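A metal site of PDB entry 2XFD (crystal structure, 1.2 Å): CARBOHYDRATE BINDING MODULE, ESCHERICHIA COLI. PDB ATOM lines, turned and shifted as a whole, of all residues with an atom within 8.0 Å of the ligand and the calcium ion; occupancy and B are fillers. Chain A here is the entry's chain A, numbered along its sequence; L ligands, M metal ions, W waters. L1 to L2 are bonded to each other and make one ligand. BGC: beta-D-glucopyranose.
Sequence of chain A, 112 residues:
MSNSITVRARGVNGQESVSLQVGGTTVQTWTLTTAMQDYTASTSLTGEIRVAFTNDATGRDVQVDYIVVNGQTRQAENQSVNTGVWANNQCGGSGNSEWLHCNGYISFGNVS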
ATOM      1  N   VAL A  12      24.841   9.641  36.582  1.00  0.00           N
ATOM      2  CA  VAL A  12      23.881  10.727  36.571  1.00  0.00           C
ATOM      3  C   VAL A  12      22.530  10.344  37.169  1.00  0.00           C
ATOM      4  O   VAL A  12      21.893  11.177  37.791  1.00  0.00           O
ATOM      5  CB  VAL A  12      23.756  11.351  35.190  1.00  0.00           C
ATOM      6  CG1 VAL A  12      25.036  11.867  34.666  1.00  0.00           C
ATOM      7  CG2 VAL A  12      23.151  10.627  34.319  1.00  0.00           C
ATOM      8  N   GLU A  16      23.814   3.413  36.893  1.00  0.00           N
ATOM      9  CA  GLU A  16      24.906   3.103  36.041  1.00  0.00           C
ATOM     10  C   GLU A  16      25.809   2.052  36.649  1.00  0.00           C
ATOM     11  O   GLU A  16      26.124   2.056  37.841  1.00  0.00           O
ATOM     12  CB  GLU A  16      25.704   4.351  35.697  1.00  0.00           C
ATOM     13  CG  GLU A  16      24.900   5.402  34.970  1.00  0.00           C
ATOM     14  CD  GLU A  16      24.097   6.377  35.803  1.00  0.00           C
ATOM     15  OE1 GLU A  16      23.983   6.189  37.052  1.00  0.00           O
ATOM     16  OE2 GLU A  16      23.575   7.383  35.191  1.00  0.00           O
ATOM     17  N   PHE A  53      31.854   1.600  31.058  1.00  0.00           N
ATOM     18  CA  PHE A  53      30.416   1.783  31.319  1.00  0.00           C
ATOM     19  C   PHE A  53      29.705   0.761  30.435  1.00  0.00           C
ATOM     20  O   PHE A  53      29.962   0.706  29.242  1.00  0.00           O
ATOM     21  CB  PHE A  53      30.025   3.209  30.930  1.00  0.00           C
ATOM     22  CG  PHE A  53      28.566   3.580  30.958  1.00  0.00           C
ATOM     23  CD1 PHE A  53      27.652   3.095  31.904  1.00  0.00           C
ATOM     24  CD2 PHE A  53      28.127   4.541  30.086  1.00  0.00           C
ATOM     25  CE1 PHE A  53      26.333   3.531  31.924  1.00  0.00           C
ATOM     26  CE2 PHE A  53      26.830   5.012  30.112  1.00  0.00           C
ATOM     27  CZ  PHE A  53      25.924   4.523  31.047  1.00  0.00           C
ATOM     28  N   ASN A  55      26.032  -0.406  30.871  1.00  0.00           N
ATOM     29  CA  ASN A  55      24.572  -0.480  30.856  1.00  0.00           C
ATOM     30  C   ASN A  55      23.903   0.808  30.432  1.00  0.00           C
ATOM     31  O   ASN A  55      22.884   1.210  31.014  1.00  0.00           O
ATOM     32  CB  ASN A  55      24.039  -1.043  32.188  1.00  0.00           C
ATOM     33  CG  ASN A  55      24.192  -0.080  33.319  1.00  0.00           C
ATOM     34  OD1 ASN A  55      25.052   0.822  33.242  1.00  0.00           O
ATOM     35  ND2 ASN A  55      23.414  -0.242  34.372  1.00  0.00           N
ATOM     36  N   ASP A  56      24.454   1.463  29.450  1.00  0.00           N
ATOM     37  CA  ASP A  56      23.874   2.670  28.918  1.00  0.00           C
ATOM     38  C   ASP A  56      22.396   2.434  28.569  1.00  0.00           C
ATOM     39  O   ASP A  56      22.015   1.355  28.069  1.00  0.00           O
ATOM     40  CB  ASP A  56      24.637   3.136  27.684  1.00  0.00           C
ATOM     41  CG  ASP A  56      24.225   4.464  27.205  1.00  0.00           C
ATOM     42  OD1 ASP A  56      23.851   5.326  28.024  1.00  0.00           O
ATOM     43  OD2 ASP A  56      24.321   4.691  25.975  1.00  0.00           O
ATOM     44  N   ALA A  57      21.618   3.477  28.769  1.00  0.00           N
ATOM     45  CA  ALA A  57      20.176   3.523  28.533  1.00  0.00           C
ATOM     46  C   ALA A  57      19.800   4.957  28.667  1.00  0.00           C
ATOM     47  O   ALA A  57      20.553   5.831  29.109  1.00  0.00           O
ATOM     48  CB  ALA A  57      19.429   2.713  29.489  1.00  0.00           C
ATOM     49  N   THR A  58      18.518   5.218  28.395  1.00  0.00           N
ATOM     50  CA  THR A  58      17.961   6.520  28.643  1.00  0.00           C
ATOM     51  C   THR A  58      18.276   7.012  30.046  1.00  0.00           C
ATOM     52  O   THR A  58      18.034   6.297  31.017  1.00  0.00           O
ATOM     53  CB  THR A  58      16.403   6.446  28.467  1.00  0.00           C
ATOM     54  OG1 THR A  58      16.187   6.079  27.134  1.00  0.00           O
ATOM     55  CG2 THR A  58      15.765   7.804  28.810  1.00  0.00           C
ATOM     56  N   GLY A  59      18.771   8.236  30.187  1.00  0.00           N
ATOM     57  CA  GLY A  59      19.008   8.851  31.496  1.00  0.00           C
ATOM     58  C   GLY A  59      20.291   8.461  32.184  1.00  0.00           C
ATOM     59  O   GLY A  59      20.564   8.984  33.278  1.00  0.00           O
ATOM     60  N   ARG A  60      21.050   7.527  31.599  1.00  0.00           N
ATOM     61  CA  ARG A  60      22.255   7.010  32.237  1.00  0.00           C
ATOM     62  C   ARG A  60      23.534   7.460  31.513  1.00  0.00           C
ATOM     63  O   ARG A  60      23.646   7.317  30.295  1.00  0.00           O
ATOM     64  CB  ARG A  60      22.268   5.504  32.193  1.00  0.00           C
ATOM     65  CG  ARG A  60      21.127   4.802  32.924  1.00  0.00           C
ATOM     66  CD  ARG A  60      21.290   3.316  32.866  1.00  0.00           C
ATOM     67  NE  ARG A  60      20.143   2.620  33.444  1.00  0.00           N
ATOM     68  CZ  ARG A  60      19.847   1.356  33.297  1.00  0.00           C
ATOM     69  NH1 ARG A  60      20.560   0.570  32.541  1.00  0.00           N
ATOM     70  NH2 ARG A  60      18.754   0.888  33.879  1.00  0.00           N
ATOM     71  N   ASP A  61      24.468   8.015  32.284  1.00  0.00           N
ATOM     72  CA  ASP A  61      25.784   8.461  31.826  1.00  0.00           C
ATOM     73  C   ASP A  61      26.733   8.358  33.032  1.00  0.00           C
ATOM     74  O   ASP A  61      26.281   8.422  34.178  1.00  0.00           O
ATOM     75  CB  ASP A  61      25.738   9.944  31.366  1.00  0.00           C
ATOM     76  CG  ASP A  61      24.903  10.201  30.162  1.00  0.00           C
ATOM     77  OD1 ASP A  61      24.100  11.181  30.228  1.00  0.00           O
ATOM     78  OD2 ASP A  61      25.058   9.497  29.156  1.00  0.00           O
ATOM     79  N   VAL A  62      28.039   8.249  32.747  1.00  0.00           N
ATOM     80  CA  VAL A  62      29.052   8.132  33.801  1.00  0.00           C
ATOM     81  C   VAL A  62      30.063   9.260  33.685  1.00  0.00           C
ATOM     82  O   VAL A  62      30.505   9.606  32.576  1.00  0.00           O
ATOM     83  CB  VAL A  62      29.735   6.772  33.702  1.00  0.00           C
ATOM     84  CG1 VAL A  62      30.957   6.685  34.625  1.00  0.00           C
ATOM     85  CG2 VAL A  62      28.734   5.632  34.005  1.00  0.00           C
ATOM     86  N   GLY A  84      33.584   5.972  24.943  1.00  0.00           N
ATOM     87  CA  GLY A  84      32.211   6.276  25.322  1.00  0.00           C
ATOM     88  C   GLY A  84      31.767   7.710  25.291  1.00  0.00           C
ATOM     89  O   GLY A  84      30.571   7.985  25.360  1.00  0.00           O
ATOM     90  N   VAL A  85      32.684   8.659  25.276  1.00  0.00           N
ATOM     91  CA  VAL A  85      32.294  10.075  25.278  1.00  0.00           C
ATOM     92  C   VAL A  85      31.513  10.376  24.019  1.00  0.00           C
ATOM     93  O   VAL A  85      31.875   9.955  22.925  1.00  0.00           O
ATOM     94  CB  VAL A  85      33.503  11.008  25.453  1.00  0.00           C
ATOM     95  CG1 VAL A  85      34.523  10.902  24.357  1.00  0.00           C
ATOM     96  CG2 VAL A  85      33.050  12.395  25.635  1.00  0.00           C
ATOM     97  N   TRP A  86      30.423  11.182  24.152  1.00  0.00           N
ATOM     98  CA  TRP A  86      29.727  11.687  22.999  1.00  0.00           C
ATOM     99  C   TRP A  86      30.440  12.969  22.608  1.00  0.00           C
ATOM    100  O   TRP A  86      30.415  13.988  23.284  1.00  0.00           O
ATOM    101  CB  TRP A  86      28.279  11.955  23.346  1.00  0.00           C
ATOM    102  CG  TRP A  86      27.476  12.373  22.142  1.00  0.00           C
ATOM    103  CD1 TRP A  86      27.098  13.659  21.805  1.00  0.00           C
ATOM    104  CD2 TRP A  86      26.967  11.519  21.148  1.00  0.00           C
ATOM    105  NE1 TRP A  86      26.392  13.622  20.636  1.00  0.00           N
ATOM    106  CE2 TRP A  86      26.248  12.322  20.217  1.00  0.00           C
ATOM    107  CE3 TRP A  86      26.976  10.158  20.951  1.00  0.00           C
ATOM    108  CZ2 TRP A  86      25.678  11.793  19.072  1.00  0.00           C
ATOM    109  CZ3 TRP A  86      26.362   9.629  19.865  1.00  0.00           C
ATOM    110  CH2 TRP A  86      25.712  10.450  18.919  1.00  0.00           C
ATOM    111  N   ALA A  87      31.092  12.955  21.442  1.00  0.00           N
ATOM    112  CA  ALA A  87      31.903  14.064  20.956  1.00  0.00           C
ATOM    113  C   ALA A  87      31.923  14.003  19.426  1.00  0.00           C
ATOM    114  O   ALA A  87      31.910  12.886  18.889  1.00  0.00           O
ATOM    115  CB  ALA A  87      33.314  14.001  21.482  1.00  0.00           C
ATOM    116  N   ASN A  89      29.414  14.329  17.508  1.00  0.00           N
ATOM    117  CA  ASN A  89      28.226  13.592  17.115  1.00  0.00           C
ATOM    118  C   ASN A  89      28.356  12.086  17.036  1.00  0.00           C
ATOM    119  O   ASN A  89      27.633  11.435  16.279  1.00  0.00           O
ATOM    120  CB  ASN A  89      27.649  14.222  15.836  1.00  0.00           C
ATOM    121  CG  ASN A  89      27.448  15.736  15.996  1.00  0.00           C
ATOM    122  OD1 ASN A  89      28.118  16.538  15.364  1.00  0.00           O
ATOM    123  ND2 ASN A  89      26.551  16.118  16.884  1.00  0.00           N
ATOM    124  N   GLN A  90      29.248  11.504  17.863  1.00  0.00           N
ATOM    125  CA  GLN A  90      29.349  10.108  17.874  1.00  0.00           C
ATOM    126  C   GLN A  90      29.980   9.667  19.171  1.00  0.00           C
ATOM    127  O   GLN A  90      30.725  10.412  19.836  1.00  0.00           O
ATOM    128  CB  GLN A  90      30.217   9.697  16.719  1.00  0.00           C
ATOM    129  CG  GLN A  90      31.617  10.151  16.863  1.00  0.00           C
ATOM    130  CD  GLN A  90      32.324  10.178  15.546  1.00  0.00           C
ATOM    131  OE1 GLN A  90      32.776   9.184  15.105  1.00  0.00           O
ATOM    132  NE2 GLN A  90      32.322  11.325  14.877  1.00  0.00           N
ATOM    133  N   CYS A  91      29.771   8.395  19.470  1.00  0.00           N
ATOM    134  CA  CYS A  91      30.446   7.805  20.626  1.00  0.00           C
ATOM    135  C   CYS A  91      31.928   7.655  20.305  1.00  0.00           C
ATOM    136  O   CYS A  91      32.303   7.180  19.240  1.00  0.00           O
ATOM    137  CB  CYS A  91      29.871   6.431  20.908  1.00  0.00           C
ATOM    138  SG  CYS A  91      28.046   6.354  21.160  1.00  0.00           S
ATOM    139  N   TRP A  99      33.853  11.811  30.708  1.00  0.00           N
ATOM    140  CA  TRP A  99      32.515  11.277  30.491  1.00  0.00           C
ATOM    141  C   TRP A  99      32.507  10.006  29.635  1.00  0.00           C
ATOM    142  O   TRP A  99      33.163   9.920  28.615  1.00  0.00           O
ATOM    143  CB  TRP A  99      31.675  12.362  29.798  1.00  0.00           C
ATOM    144  CG  TRP A  99      31.320  13.442  30.767  1.00  0.00           C
ATOM    145  CD1 TRP A  99      32.028  14.558  31.033  1.00  0.00           C
ATOM    146  CD2 TRP A  99      30.229  13.427  31.690  1.00  0.00           C
ATOM    147  NE1 TRP A  99      31.438  15.307  32.016  1.00  0.00           N
ATOM    148  CE2 TRP A  99      30.306  14.638  32.442  1.00  0.00           C
ATOM    149  CE3 TRP A  99      29.147  12.554  31.943  1.00  0.00           C
ATOM    150  CZ2 TRP A  99      29.369  14.954  33.437  1.00  0.00           C
ATOM    151  CZ3 TRP A  99      28.256  12.908  32.896  1.00  0.00           C
ATOM    152  CH2 TRP A  99      28.380  14.121  33.620  1.00  0.00           C
ATOM    153  N   LEU A 100      31.612   9.145  30.046  1.00  0.00           N
ATOM    154  CA  LEU A 100      31.178   8.001  29.242  1.00  0.00           C
ATOM    155  C   LEU A 100      29.685   8.157  29.077  1.00  0.00           C
ATOM    156  O   LEU A 100      28.880   7.881  29.973  1.00  0.00           O
ATOM    157  CB  LEU A 100      31.520   6.679  29.909  1.00  0.00           C
ATOM    158  CG  LEU A 100      33.017   6.382  30.042  1.00  0.00           C
ATOM    159  CD1 LEU A 100      33.275   5.279  31.032  1.00  0.00           C
ATOM    160  CD2 LEU A 100      33.611   6.086  28.646  1.00  0.00           C
ATOM    161  N   HIS A 101      29.276   8.622  27.886  1.00  0.00           N
ATOM    162  CA  HIS A 101      27.845   8.786  27.539  1.00  0.00           C
ATOM    163  C   HIS A 101      27.283   7.515  26.972  1.00  0.00           C
ATOM    164  O   HIS A 101      26.117   7.130  27.217  1.00  0.00           O
ATOM    165  CB  HIS A 101      27.681   9.942  26.572  1.00  0.00           C
ATOM    166  CG  HIS A 101      28.157  11.237  27.096  1.00  0.00           C
ATOM    167  ND1 HIS A 101      27.525  12.039  28.053  1.00  0.00           N
ATOM    168  CD2 HIS A 101      29.255  11.906  26.728  1.00  0.00           C
ATOM    169  CE1 HIS A 101      28.242  13.152  28.201  1.00  0.00           C
ATOM    170  NE2 HIS A 101      29.305  13.061  27.418  1.00  0.00           N
ATOM    171  N   CYS A 102      28.051   6.879  26.130  1.00  0.00           N
ATOM    172  CA  CYS A 102      27.714   5.609  25.494  1.00  0.00           C
ATOM    173  C   CYS A 102      28.441   4.488  26.267  1.00  0.00           C
ATOM    174  O   CYS A 102      29.439   4.746  26.931  1.00  0.00           O
ATOM    175  CB  CYS A 102      28.185   5.587  24.039  1.00  0.00           C
ATOM    176  SG  CYS A 102      27.756   7.026  23.099  1.00  0.00           S
ATOM    177  N   ASN A 103      27.989   3.264  26.068  1.00  0.00           N
ATOM    178  CA  ASN A 103      28.808   2.141  26.465  1.00  0.00           C
ATOM    179  C   ASN A 103      30.215   2.276  25.859  1.00  0.00           C
ATOM    180  O   ASN A 103      30.330   2.613  24.693  1.00  0.00           O
ATOM    181  CB  ASN A 103      28.205   0.790  26.084  1.00  0.00           C
ATOM    182  CG  ASN A 103      26.987   0.429  26.897  1.00  0.00           C
ATOM    183  OD1 ASN A 103      26.874   0.801  28.070  1.00  0.00           O
ATOM    184  ND2 ASN A 103      26.075  -0.269  26.254  1.00  0.00           N
HETATM  185  C2  BGC L   1      22.861  14.362  21.958  1.00  0.00           C
HETATM  186  C3  BGC L   1      22.605  13.011  22.584  1.00  0.00           C
HETATM  187  C4  BGC L   1      23.738  12.572  23.490  1.00  0.00           C
HETATM  188  C5  BGC L   1      24.110  13.686  24.387  1.00  0.00           C
HETATM  189  C6  BGC L   1      25.240  13.275  25.252  1.00  0.00           C
HETATM  190  C1  BGC L   1      23.204  15.335  23.074  1.00  0.00           C
HETATM  191  O1  BGC L   1      23.354  16.676  22.680  1.00  0.00           O
HETATM  192  O2  BGC L   1      21.742  14.769  21.191  1.00  0.00           O
HETATM  193  O3  BGC L   1      22.404  12.029  21.574  1.00  0.00           O
HETATM  194  O4  BGC L   1      23.252  11.594  24.267  1.00  0.00           O
HETATM  195  O5  BGC L   1      24.429  14.863  23.607  1.00  0.00           O
HETATM  196  O6  BGC L   1      25.635  14.332  26.082  1.00  0.00           O
HETATM  197  C2  BGC L   2      23.480   9.348  25.045  1.00  0.00           C
HETATM  198  C3  BGC L   2      23.872   7.931  24.676  1.00  0.00           C
HETATM  199  C4  BGC L   2      23.262   7.504  23.324  1.00  0.00           C
HETATM  200  C5  BGC L   2      23.662   8.541  22.287  1.00  0.00           C
HETATM  201  C6  BGC L   2      23.176   8.318  20.842  1.00  0.00           C
HETATM  202  C1  BGC L   2      23.769  10.297  23.924  1.00  0.00           C
HETATM  203  O2  BGC L   2      24.128   9.653  26.300  1.00  0.00           O
HETATM  204  O3  BGC L   2      23.384   7.063  25.712  1.00  0.00           O
HETATM  205  O4  BGC L   2      23.763   6.264  22.907  1.00  0.00           O
HETATM  206  O5  BGC L   2      23.213   9.797  22.713  1.00  0.00           O
HETATM  207  O6  BGC L   2      21.762   8.340  20.882  1.00  0.00           O
HETATM  208 CA    CA M   1      24.016   7.741  27.999  1.00  0.00          CA
HETATM  209  O   HOH W   1      23.479  11.859  27.653  1.00  0.00           O
HETATM  210  O   HOH W   2      21.680   8.204  28.100  1.00  0.00           O
HETATM  211  O   HOH W   3      24.611   5.455  20.658  1.00  0.00           O
HETATM  212  O   HOH W   4      20.603   6.501  25.740  1.00  0.00           O
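N of His 101 sits at hydrogen-bond distance from O of Gly 84 (2.9 Å).
O of Asp 61 lies within hydrogen-bond range of N of Val 12.
N of Asp 61 sits at hydrogen-bond distance from OE2 of Glu 16 (3.1 Å).
The guanidinium group (NH1) of Arg 60 lies within hydrogen-bond range of the backbone carbonyl oxygen (O) of Asn 55, at 2.9 Å.
The side-chain amide oxygen of Asn 103 is in hydrogen-bond range of the backbone NH of Asp 56, at 2.9 Å.
The side-chain sulfur of Cys 102 forms a disulfide with the side-chain sulfur of Cys 91, 2.1 Å away.
CD1 of Trp 86 touches O5 of BGC L1, 3.4 Å away.
Hydrophobic or aromatic side chains within 4 Å of the ligand: Trp 86 and His 101.
Of the 23 residues printed, 4 come within 4 Å of the ligand.
Of the 23 residues printed, 4 come within 4 Å of the calcium ion.
The nearest printed residue that does not touch the calcium ion is Ala 57 (4.1 Å).
O of His 101 binds the calcium ion (2.3 Å).
The side-chain carboxylate (OD2) of Asp 61 binds the calcium ion, 2.3 Å away.
The calcium ion is bound by the backbone carbonyl oxygen (O) of Arg 60 (2.4 Å).
The calcium ion is bound by water W2 (2.4 Å).
OD1 of Asp 56 is bound to the calcium ion, 2.4 Å away.
The calcium ion is bound by O3 of BGC L2, at 2.5 Å.
The calcium ion is bound by O2 of BGC L2 (2.6 Å).
The calcium ion has seven donor atoms within binding distance.
Water W3 bridges O4 of BGC L2 (2.5 Å) and SG of Cys 91 (3.6 Å).
Water W1 bridges the side-chain carboxylate (OD1) of Asp 61 (2.7 Å) and an oxygen (O4) of BGC L1 (3.4 Å).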
